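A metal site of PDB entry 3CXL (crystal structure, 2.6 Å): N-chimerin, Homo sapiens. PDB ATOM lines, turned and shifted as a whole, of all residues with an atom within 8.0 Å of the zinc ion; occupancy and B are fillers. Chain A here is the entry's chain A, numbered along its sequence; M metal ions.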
ATOM      1  N   LEU A  24     -13.389   9.805  -4.862  1.00  0.00           N
ATOM      2  CA  LEU A  24     -14.275   8.856  -4.186  1.00  0.00           C
ATOM      3  C   LEU A  24     -13.516   7.733  -3.491  1.00  0.00           C
ATOM      4  O   LEU A  24     -14.053   7.132  -2.565  1.00  0.00           O
ATOM      5  CB  LEU A  24     -15.333   8.298  -5.155  1.00  0.00           C
ATOM      6  CG  LEU A  24     -16.254   9.355  -5.785  1.00  0.00           C
ATOM      7  CD1 LEU A  24     -17.362   8.732  -6.625  1.00  0.00           C
ATOM      8  CD2 LEU A  24     -16.859  10.298  -4.731  1.00  0.00           C
ATOM      9  N   ILE A 138     -20.995  13.294  -7.521  1.00  0.00           N
ATOM     10  CA  ILE A 138     -21.517  12.041  -8.039  1.00  0.00           C
ATOM     11  C   ILE A 138     -22.603  12.305  -9.078  1.00  0.00           C
ATOM     12  O   ILE A 138     -22.681  11.628 -10.118  1.00  0.00           O
ATOM     13  CB  ILE A 138     -22.050  11.176  -6.941  1.00  0.00           C
ATOM     14  CG1 ILE A 138     -20.889  10.686  -6.037  1.00  0.00           C
ATOM     15  CG2 ILE A 138     -22.791   9.982  -7.534  1.00  0.00           C
ATOM     16  CD1 ILE A 138     -21.321  10.156  -4.707  1.00  0.00           C
ATOM     17  N   MET A 141     -20.409  13.146 -12.044  1.00  0.00           N
ATOM     18  CA  MET A 141     -19.220  12.291 -12.404  1.00  0.00           C
ATOM     19  C   MET A 141     -19.192  11.973 -13.845  1.00  0.00           C
ATOM     20  O   MET A 141     -18.142  11.702 -14.383  1.00  0.00           O
ATOM     21  CB  MET A 141     -19.246  10.898 -11.761  1.00  0.00           C
ATOM     22  CG  MET A 141     -19.548  10.767 -10.351  1.00  0.00           C
ATOM     23  SD  MET A 141     -19.218   9.094  -9.736  1.00  0.00           S
ATOM     24  CE  MET A 141     -20.145   8.079 -10.876  1.00  0.00           C
ATOM     25  N   THR A 142     -20.381  11.915 -14.460  1.00  0.00           N
ATOM     26  CA  THR A 142     -20.589  11.318 -15.776  1.00  0.00           C
ATOM     27  C   THR A 142     -20.502  12.269 -16.959  1.00  0.00           C
ATOM     28  O   THR A 142     -20.591  11.822 -18.093  1.00  0.00           O
ATOM     29  CB  THR A 142     -21.980  10.637 -15.828  1.00  0.00           C
ATOM     30  OG1 THR A 142     -22.995  11.628 -15.714  1.00  0.00           O
ATOM     31  CG2 THR A 142     -22.119   9.618 -14.713  1.00  0.00           C
ATOM     32  N   PRO A 145     -17.124  11.589 -20.159  1.00  0.00           N
ATOM     33  CA  PRO A 145     -16.668  10.244 -19.836  1.00  0.00           C
ATOM     34  C   PRO A 145     -15.455   9.823 -20.656  1.00  0.00           C
ATOM     35  O   PRO A 145     -15.194  10.383 -21.710  1.00  0.00           O
ATOM     36  CB  PRO A 145     -17.887   9.381 -20.176  1.00  0.00           C
ATOM     37  CG  PRO A 145     -18.575  10.134 -21.279  1.00  0.00           C
ATOM     38  CD  PRO A 145     -18.316  11.592 -21.028  1.00  0.00           C
ATOM     39  N   TRP A 222     -11.917   0.684 -10.517  1.00  0.00           N
ATOM     40  CA  TRP A 222     -12.450   1.955 -10.976  1.00  0.00           C
ATOM     41  C   TRP A 222     -13.435   1.721 -12.101  1.00  0.00           C
ATOM     42  O   TRP A 222     -13.337   0.755 -12.801  1.00  0.00           O
ATOM     43  CB  TRP A 222     -11.302   2.877 -11.430  1.00  0.00           C
ATOM     44  CG  TRP A 222     -10.679   3.689 -10.296  1.00  0.00           C
ATOM     45  CD1 TRP A 222     -10.759   5.045 -10.124  1.00  0.00           C
ATOM     46  CD2 TRP A 222      -9.897   3.195  -9.204  1.00  0.00           C
ATOM     47  NE1 TRP A 222     -10.070   5.416  -8.986  1.00  0.00           N
ATOM     48  CE2 TRP A 222      -9.532   4.294  -8.407  1.00  0.00           C
ATOM     49  CE3 TRP A 222      -9.476   1.913  -8.818  1.00  0.00           C
ATOM     50  CZ2 TRP A 222      -8.769   4.161  -7.249  1.00  0.00           C
ATOM     51  CZ3 TRP A 222      -8.707   1.789  -7.679  1.00  0.00           C
ATOM     52  CH2 TRP A 222      -8.364   2.901  -6.909  1.00  0.00           C
ATOM     53  N   CYS A 223     -14.406   2.617 -12.246  1.00  0.00           N
ATOM     54  CA  CYS A 223     -15.399   2.536 -13.330  1.00  0.00           C
ATOM     55  C   CYS A 223     -14.803   2.906 -14.690  1.00  0.00           C
ATOM     56  O   CYS A 223     -14.197   3.993 -14.830  1.00  0.00           O
ATOM     57  CB  CYS A 223     -16.560   3.478 -13.030  1.00  0.00           C
ATOM     58  SG  CYS A 223     -17.681   3.847 -14.416  1.00  0.00           S
ATOM     59  N   GLU A 224     -14.996   2.038 -15.691  1.00  0.00           N
ATOM     60  CA  GLU A 224     -14.429   2.251 -17.029  1.00  0.00           C
ATOM     61  C   GLU A 224     -15.337   3.073 -17.936  1.00  0.00           C
ATOM     62  O   GLU A 224     -15.160   3.093 -19.165  1.00  0.00           O
ATOM     63  CB  GLU A 224     -14.133   0.915 -17.747  1.00  0.00           C
ATOM     64  CG  GLU A 224     -13.330  -0.123 -16.973  1.00  0.00           C
ATOM     65  CD  GLU A 224     -13.388  -1.489 -17.660  1.00  0.00           C
ATOM     66  OE1 GLU A 224     -12.856  -1.616 -18.800  1.00  0.00           O
ATOM     67  OE2 GLU A 224     -13.980  -2.427 -17.094  1.00  0.00           O
ATOM     68  N   TYR A 225     -16.326   3.750 -17.362  1.00  0.00           N
ATOM     69  CA  TYR A 225     -17.118   4.708 -18.154  1.00  0.00           C
ATOM     70  C   TYR A 225     -16.807   6.127 -17.751  1.00  0.00           C
ATOM     71  O   TYR A 225     -16.545   6.972 -18.603  1.00  0.00           O
ATOM     72  CB  TYR A 225     -18.607   4.456 -18.011  1.00  0.00           C
ATOM     73  CG  TYR A 225     -19.462   5.459 -18.752  1.00  0.00           C
ATOM     74  CD1 TYR A 225     -19.653   5.370 -20.149  1.00  0.00           C
ATOM     75  CD2 TYR A 225     -20.060   6.506 -18.074  1.00  0.00           C
ATOM     76  CE1 TYR A 225     -20.416   6.306 -20.830  1.00  0.00           C
ATOM     77  CE2 TYR A 225     -20.840   7.440 -18.754  1.00  0.00           C
ATOM     78  CZ  TYR A 225     -20.997   7.337 -20.132  1.00  0.00           C
ATOM     79  OH  TYR A 225     -21.756   8.266 -20.763  1.00  0.00           O
ATOM     80  N   CYS A 226     -16.867   6.393 -16.446  1.00  0.00           N
ATOM     81  CA  CYS A 226     -16.686   7.729 -15.892  1.00  0.00           C
ATOM     82  C   CYS A 226     -15.387   7.867 -15.103  1.00  0.00           C
ATOM     83  O   CYS A 226     -15.100   8.930 -14.578  1.00  0.00           O
ATOM     84  CB  CYS A 226     -17.837   8.034 -14.951  1.00  0.00           C
ATOM     85  SG  CYS A 226     -17.705   7.180 -13.362  1.00  0.00           S
ATOM     86  N   ALA A 227     -14.614   6.797 -15.019  1.00  0.00           N
ATOM     87  CA  ALA A 227     -13.254   6.876 -14.473  1.00  0.00           C
ATOM     88  C   ALA A 227     -13.189   7.073 -12.954  1.00  0.00           C
ATOM     89  O   ALA A 227     -12.111   7.264 -12.423  1.00  0.00           O
ATOM     90  CB  ALA A 227     -12.466   7.974 -15.184  1.00  0.00           C
ATOM     91  N   ASN A 228     -14.335   7.026 -12.259  1.00  0.00           N
ATOM     92  CA  ASN A 228     -14.365   7.240 -10.820  1.00  0.00           C
ATOM     93  C   ASN A 228     -14.388   5.942 -10.061  1.00  0.00           C
ATOM     94  O   ASN A 228     -14.779   4.891 -10.609  1.00  0.00           O
ATOM     95  CB  ASN A 228     -15.535   8.124 -10.395  1.00  0.00           C
ATOM     96  CG  ASN A 228     -15.266   9.604 -10.617  1.00  0.00           C
ATOM     97  OD1 ASN A 228     -14.718  10.278  -9.750  1.00  0.00           O
ATOM     98  ND2 ASN A 228     -15.622  10.090 -11.776  1.00  0.00           N
ATOM     99  N   PHE A 229     -13.953   6.019  -8.795  1.00  0.00           N
ATOM    100  CA  PHE A 229     -13.832   4.866  -7.919  1.00  0.00           C
ATOM    101  C   PHE A 229     -15.172   4.215  -7.715  1.00  0.00           C
ATOM    102  O   PHE A 229     -16.197   4.915  -7.609  1.00  0.00           O
ATOM    103  CB  PHE A 229     -13.259   5.268  -6.553  1.00  0.00           C
ATOM    104  CG  PHE A 229     -13.160   4.120  -5.590  1.00  0.00           C
ATOM    105  CD1 PHE A 229     -12.336   3.044  -5.860  1.00  0.00           C
ATOM    106  CD2 PHE A 229     -13.920   4.109  -4.415  1.00  0.00           C
ATOM    107  CE1 PHE A 229     -12.259   1.976  -4.995  1.00  0.00           C
ATOM    108  CE2 PHE A 229     -13.832   3.063  -3.553  1.00  0.00           C
ATOM    109  CZ  PHE A 229     -13.001   1.982  -3.838  1.00  0.00           C
ATOM    110  N   MET A 230     -15.162   2.886  -7.651  1.00  0.00           N
ATOM    111  CA  MET A 230     -16.398   2.147  -7.362  1.00  0.00           C
ATOM    112  C   MET A 230     -16.391   1.775  -5.901  1.00  0.00           C
ATOM    113  O   MET A 230     -15.705   0.881  -5.482  1.00  0.00           O
ATOM    114  CB  MET A 230     -16.526   0.926  -8.287  1.00  0.00           C
ATOM    115  CG  MET A 230     -16.765   1.326  -9.779  1.00  0.00           C
ATOM    116  SD  MET A 230     -17.241  -0.044 -10.910  1.00  0.00           S
ATOM    117  CE  MET A 230     -16.124  -1.308 -10.342  1.00  0.00           C
ATOM    118  N   TRP A 231     -17.172   2.511  -5.110  1.00  0.00           N
ATOM    119  CA  TRP A 231     -17.105   2.471  -3.638  1.00  0.00           C
ATOM    120  C   TRP A 231     -18.012   1.426  -3.028  1.00  0.00           C
ATOM    121  O   TRP A 231     -18.940   0.961  -3.667  1.00  0.00           O
ATOM    122  CB  TRP A 231     -17.453   3.843  -3.058  1.00  0.00           C
ATOM    123  CG  TRP A 231     -18.891   4.276  -3.288  1.00  0.00           C
ATOM    124  CD1 TRP A 231     -19.974   4.003  -2.497  1.00  0.00           C
ATOM    125  CD2 TRP A 231     -19.379   5.070  -4.375  1.00  0.00           C
ATOM    126  NE1 TRP A 231     -21.120   4.563  -3.036  1.00  0.00           N
ATOM    127  CE2 TRP A 231     -20.790   5.232  -4.172  1.00  0.00           C
ATOM    128  CE3 TRP A 231     -18.782   5.665  -5.488  1.00  0.00           C
ATOM    129  CZ2 TRP A 231     -21.591   5.958  -5.067  1.00  0.00           C
ATOM    130  CZ3 TRP A 231     -19.583   6.388  -6.370  1.00  0.00           C
ATOM    131  CH2 TRP A 231     -20.977   6.534  -6.148  1.00  0.00           C
ATOM    132  N   ASN A 246     -16.262  -3.174 -16.562  1.00  0.00           N
ATOM    133  CA  ASN A 246     -16.592  -2.801 -15.177  1.00  0.00           C
ATOM    134  C   ASN A 246     -17.041  -1.322 -15.027  1.00  0.00           C
ATOM    135  O   ASN A 246     -16.244  -0.387 -15.266  1.00  0.00           O
ATOM    136  CB  ASN A 246     -15.381  -3.019 -14.261  1.00  0.00           C
ATOM    137  CG  ASN A 246     -14.906  -4.442 -14.260  1.00  0.00           C
ATOM    138  OD1 ASN A 246     -15.596  -5.346 -14.735  1.00  0.00           O
ATOM    139  ND2 ASN A 246     -13.713  -4.669 -13.702  1.00  0.00           N
ATOM    140  N   VAL A 247     -18.296  -1.116 -14.605  1.00  0.00           N
ATOM    141  CA  VAL A 247     -18.894   0.217 -14.457  1.00  0.00           C
ATOM    142  C   VAL A 247     -19.828   0.304 -13.239  1.00  0.00           C
ATOM    143  O   VAL A 247     -20.131  -0.716 -12.587  1.00  0.00           O
ATOM    144  CB  VAL A 247     -19.733   0.606 -15.713  1.00  0.00           C
ATOM    145  CG1 VAL A 247     -18.847   0.708 -16.963  1.00  0.00           C
ATOM    146  CG2 VAL A 247     -20.877  -0.391 -15.921  1.00  0.00           C
ATOM    147  N   HIS A 248     -20.300   1.519 -12.960  1.00  0.00           N
ATOM    148  CA  HIS A 248     -21.318   1.758 -11.935  1.00  0.00           C
ATOM    149  C   HIS A 248     -22.689   1.378 -12.448  1.00  0.00           C
ATOM    150  O   HIS A 248     -22.949   1.529 -13.620  1.00  0.00           O
ATOM    151  CB  HIS A 248     -21.423   3.242 -11.591  1.00  0.00           C
ATOM    152  CG  HIS A 248     -20.254   3.816 -10.911  1.00  0.00           C
ATOM    153  ND1 HIS A 248     -19.283   4.537 -11.592  1.00  0.00           N
ATOM    154  CD2 HIS A 248     -19.905   3.856  -9.613  1.00  0.00           C
ATOM    155  CE1 HIS A 248     -18.382   4.976 -10.728  1.00  0.00           C
ATOM    156  NE2 HIS A 248     -18.720   4.558  -9.521  1.00  0.00           N
ATOM    157  N   LYS A 249     -23.581   0.979 -11.554  1.00  0.00           N
ATOM    158  CA  LYS A 249     -24.970   0.689 -11.873  1.00  0.00           C
ATOM    159  C   LYS A 249     -25.589   1.758 -12.779  1.00  0.00           C
ATOM    160  O   LYS A 249     -26.164   1.449 -13.826  1.00  0.00           O
ATOM    161  CB  LYS A 249     -25.794   0.568 -10.595  1.00  0.00           C
ATOM    162  CG  LYS A 249     -27.241   0.157 -10.798  1.00  0.00           C
ATOM    163  CD  LYS A 249     -27.867  -0.394  -9.495  1.00  0.00           C
ATOM    164  CE  LYS A 249     -29.400  -0.365  -9.514  1.00  0.00           C
ATOM    165  NZ  LYS A 249     -29.996  -1.143 -10.640  1.00  0.00           N
ATOM    166  N   GLN A 250     -25.474   3.031 -12.372  1.00  0.00           N
ATOM    167  CA  GLN A 250     -26.067   4.158 -13.141  1.00  0.00           C
ATOM    168  C   GLN A 250     -25.308   4.424 -14.424  1.00  0.00           C
ATOM    169  O   GLN A 250     -25.905   4.712 -15.432  1.00  0.00           O
ATOM    170  CB  GLN A 250     -26.168   5.433 -12.306  1.00  0.00           C
ATOM    171  CG  GLN A 250     -27.083   5.270 -11.128  1.00  0.00           C
ATOM    172  CD  GLN A 250     -27.310   6.573 -10.357  1.00  0.00           C
ATOM    173  OE1 GLN A 250     -26.628   7.580 -10.570  1.00  0.00           O
ATOM    174  NE2 GLN A 250     -28.277   6.550  -9.440  1.00  0.00           N
ATOM    175  N   CYS A 251     -23.985   4.298 -14.383  1.00  0.00           N
ATOM    176  CA  CYS A 251     -23.191   4.374 -15.614  1.00  0.00           C
ATOM    177  C   CYS A 251     -23.536   3.279 -16.612  1.00  0.00           C
ATOM    178  O   CYS A 251     -23.361   3.465 -17.833  1.00  0.00           O
ATOM    179  CB  CYS A 251     -21.716   4.303 -15.293  1.00  0.00           C
ATOM    180  SG  CYS A 251     -21.214   5.754 -14.405  1.00  0.00           S
ATOM    181  N   SER A 252     -24.030   2.147 -16.109  1.00  0.00           N
ATOM    182  CA  SER A 252     -24.396   1.010 -16.980  1.00  0.00           C
ATOM    183  C   SER A 252     -25.406   1.407 -18.051  1.00  0.00           C
ATOM    184  O   SER A 252     -25.316   0.960 -19.179  1.00  0.00           O
ATOM    185  CB  SER A 252     -24.951  -0.148 -16.130  1.00  0.00           C
ATOM    186  OG  SER A 252     -26.321   0.036 -15.811  1.00  0.00           O
ATOM    187  N   MET A 254     -25.661   4.208 -19.475  1.00  0.00           N
ATOM    188  CA  MET A 254     -25.085   5.214 -20.388  1.00  0.00           C
ATOM    189  C   MET A 254     -24.143   4.615 -21.417  1.00  0.00           C
ATOM    190  O   MET A 254     -23.826   5.272 -22.404  1.00  0.00           O
ATOM    191  CB  MET A 254     -24.336   6.285 -19.598  1.00  0.00           C
ATOM    192  CG  MET A 254     -25.186   7.071 -18.618  1.00  0.00           C
ATOM    193  SD  MET A 254     -24.206   8.261 -17.683  1.00  0.00           S
ATOM    194  CE  MET A 254     -25.498   8.992 -16.717  1.00  0.00           C
ATOM    195  N   VAL A 255     -23.689   3.387 -21.170  1.00  0.00           N
ATOM    196  CA  VAL A 255     -22.712   2.748 -22.047  1.00  0.00           C
ATOM    197  C   VAL A 255     -23.403   2.342 -23.346  1.00  0.00           C
ATOM    198  O   VAL A 255     -24.436   1.697 -23.296  1.00  0.00           O
ATOM    199  CB  VAL A 255     -22.119   1.474 -21.391  1.00  0.00           C
ATOM    200  CG1 VAL A 255     -21.153   0.776 -22.340  1.00  0.00           C
ATOM    201  CG2 VAL A 255     -21.431   1.820 -20.070  1.00  0.00           C
HETATM  202 ZN    ZN M   1     -19.129   5.384 -13.491  1.00  0.00          ZN
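The backbone NH (N) of Tyr 225 lies close to the side-chain sulfur (SG) of Cys 223 (3.2 Å).
O of Cys 226 sits at hydrogen-bond distance from ND2 of Asn 228.
NE2 of His 248 sits at hydrogen-bond distance from O of Phe 229, 3.2 Å away.
The backbone NH (N) of Cys 223 lies within hydrogen-bond range of the backbone carbonyl oxygen (O) of Asn 228 (2.8 Å).
The zinc ion is bound by ND1 of His 248 (2.1 Å).
SG of Cys 226 binds the zinc ion.
The zinc ion is bound by SG of Cys 223, at 2.3 Å.
The zinc ion is bound by SG of Cys 251 (2.3 Å).
Met 141 touches the zinc ion (CE to ZN, 3.9 Å).
The nearest printed residue that does not touch the zinc ion is Tyr 225 (4.6 Å).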
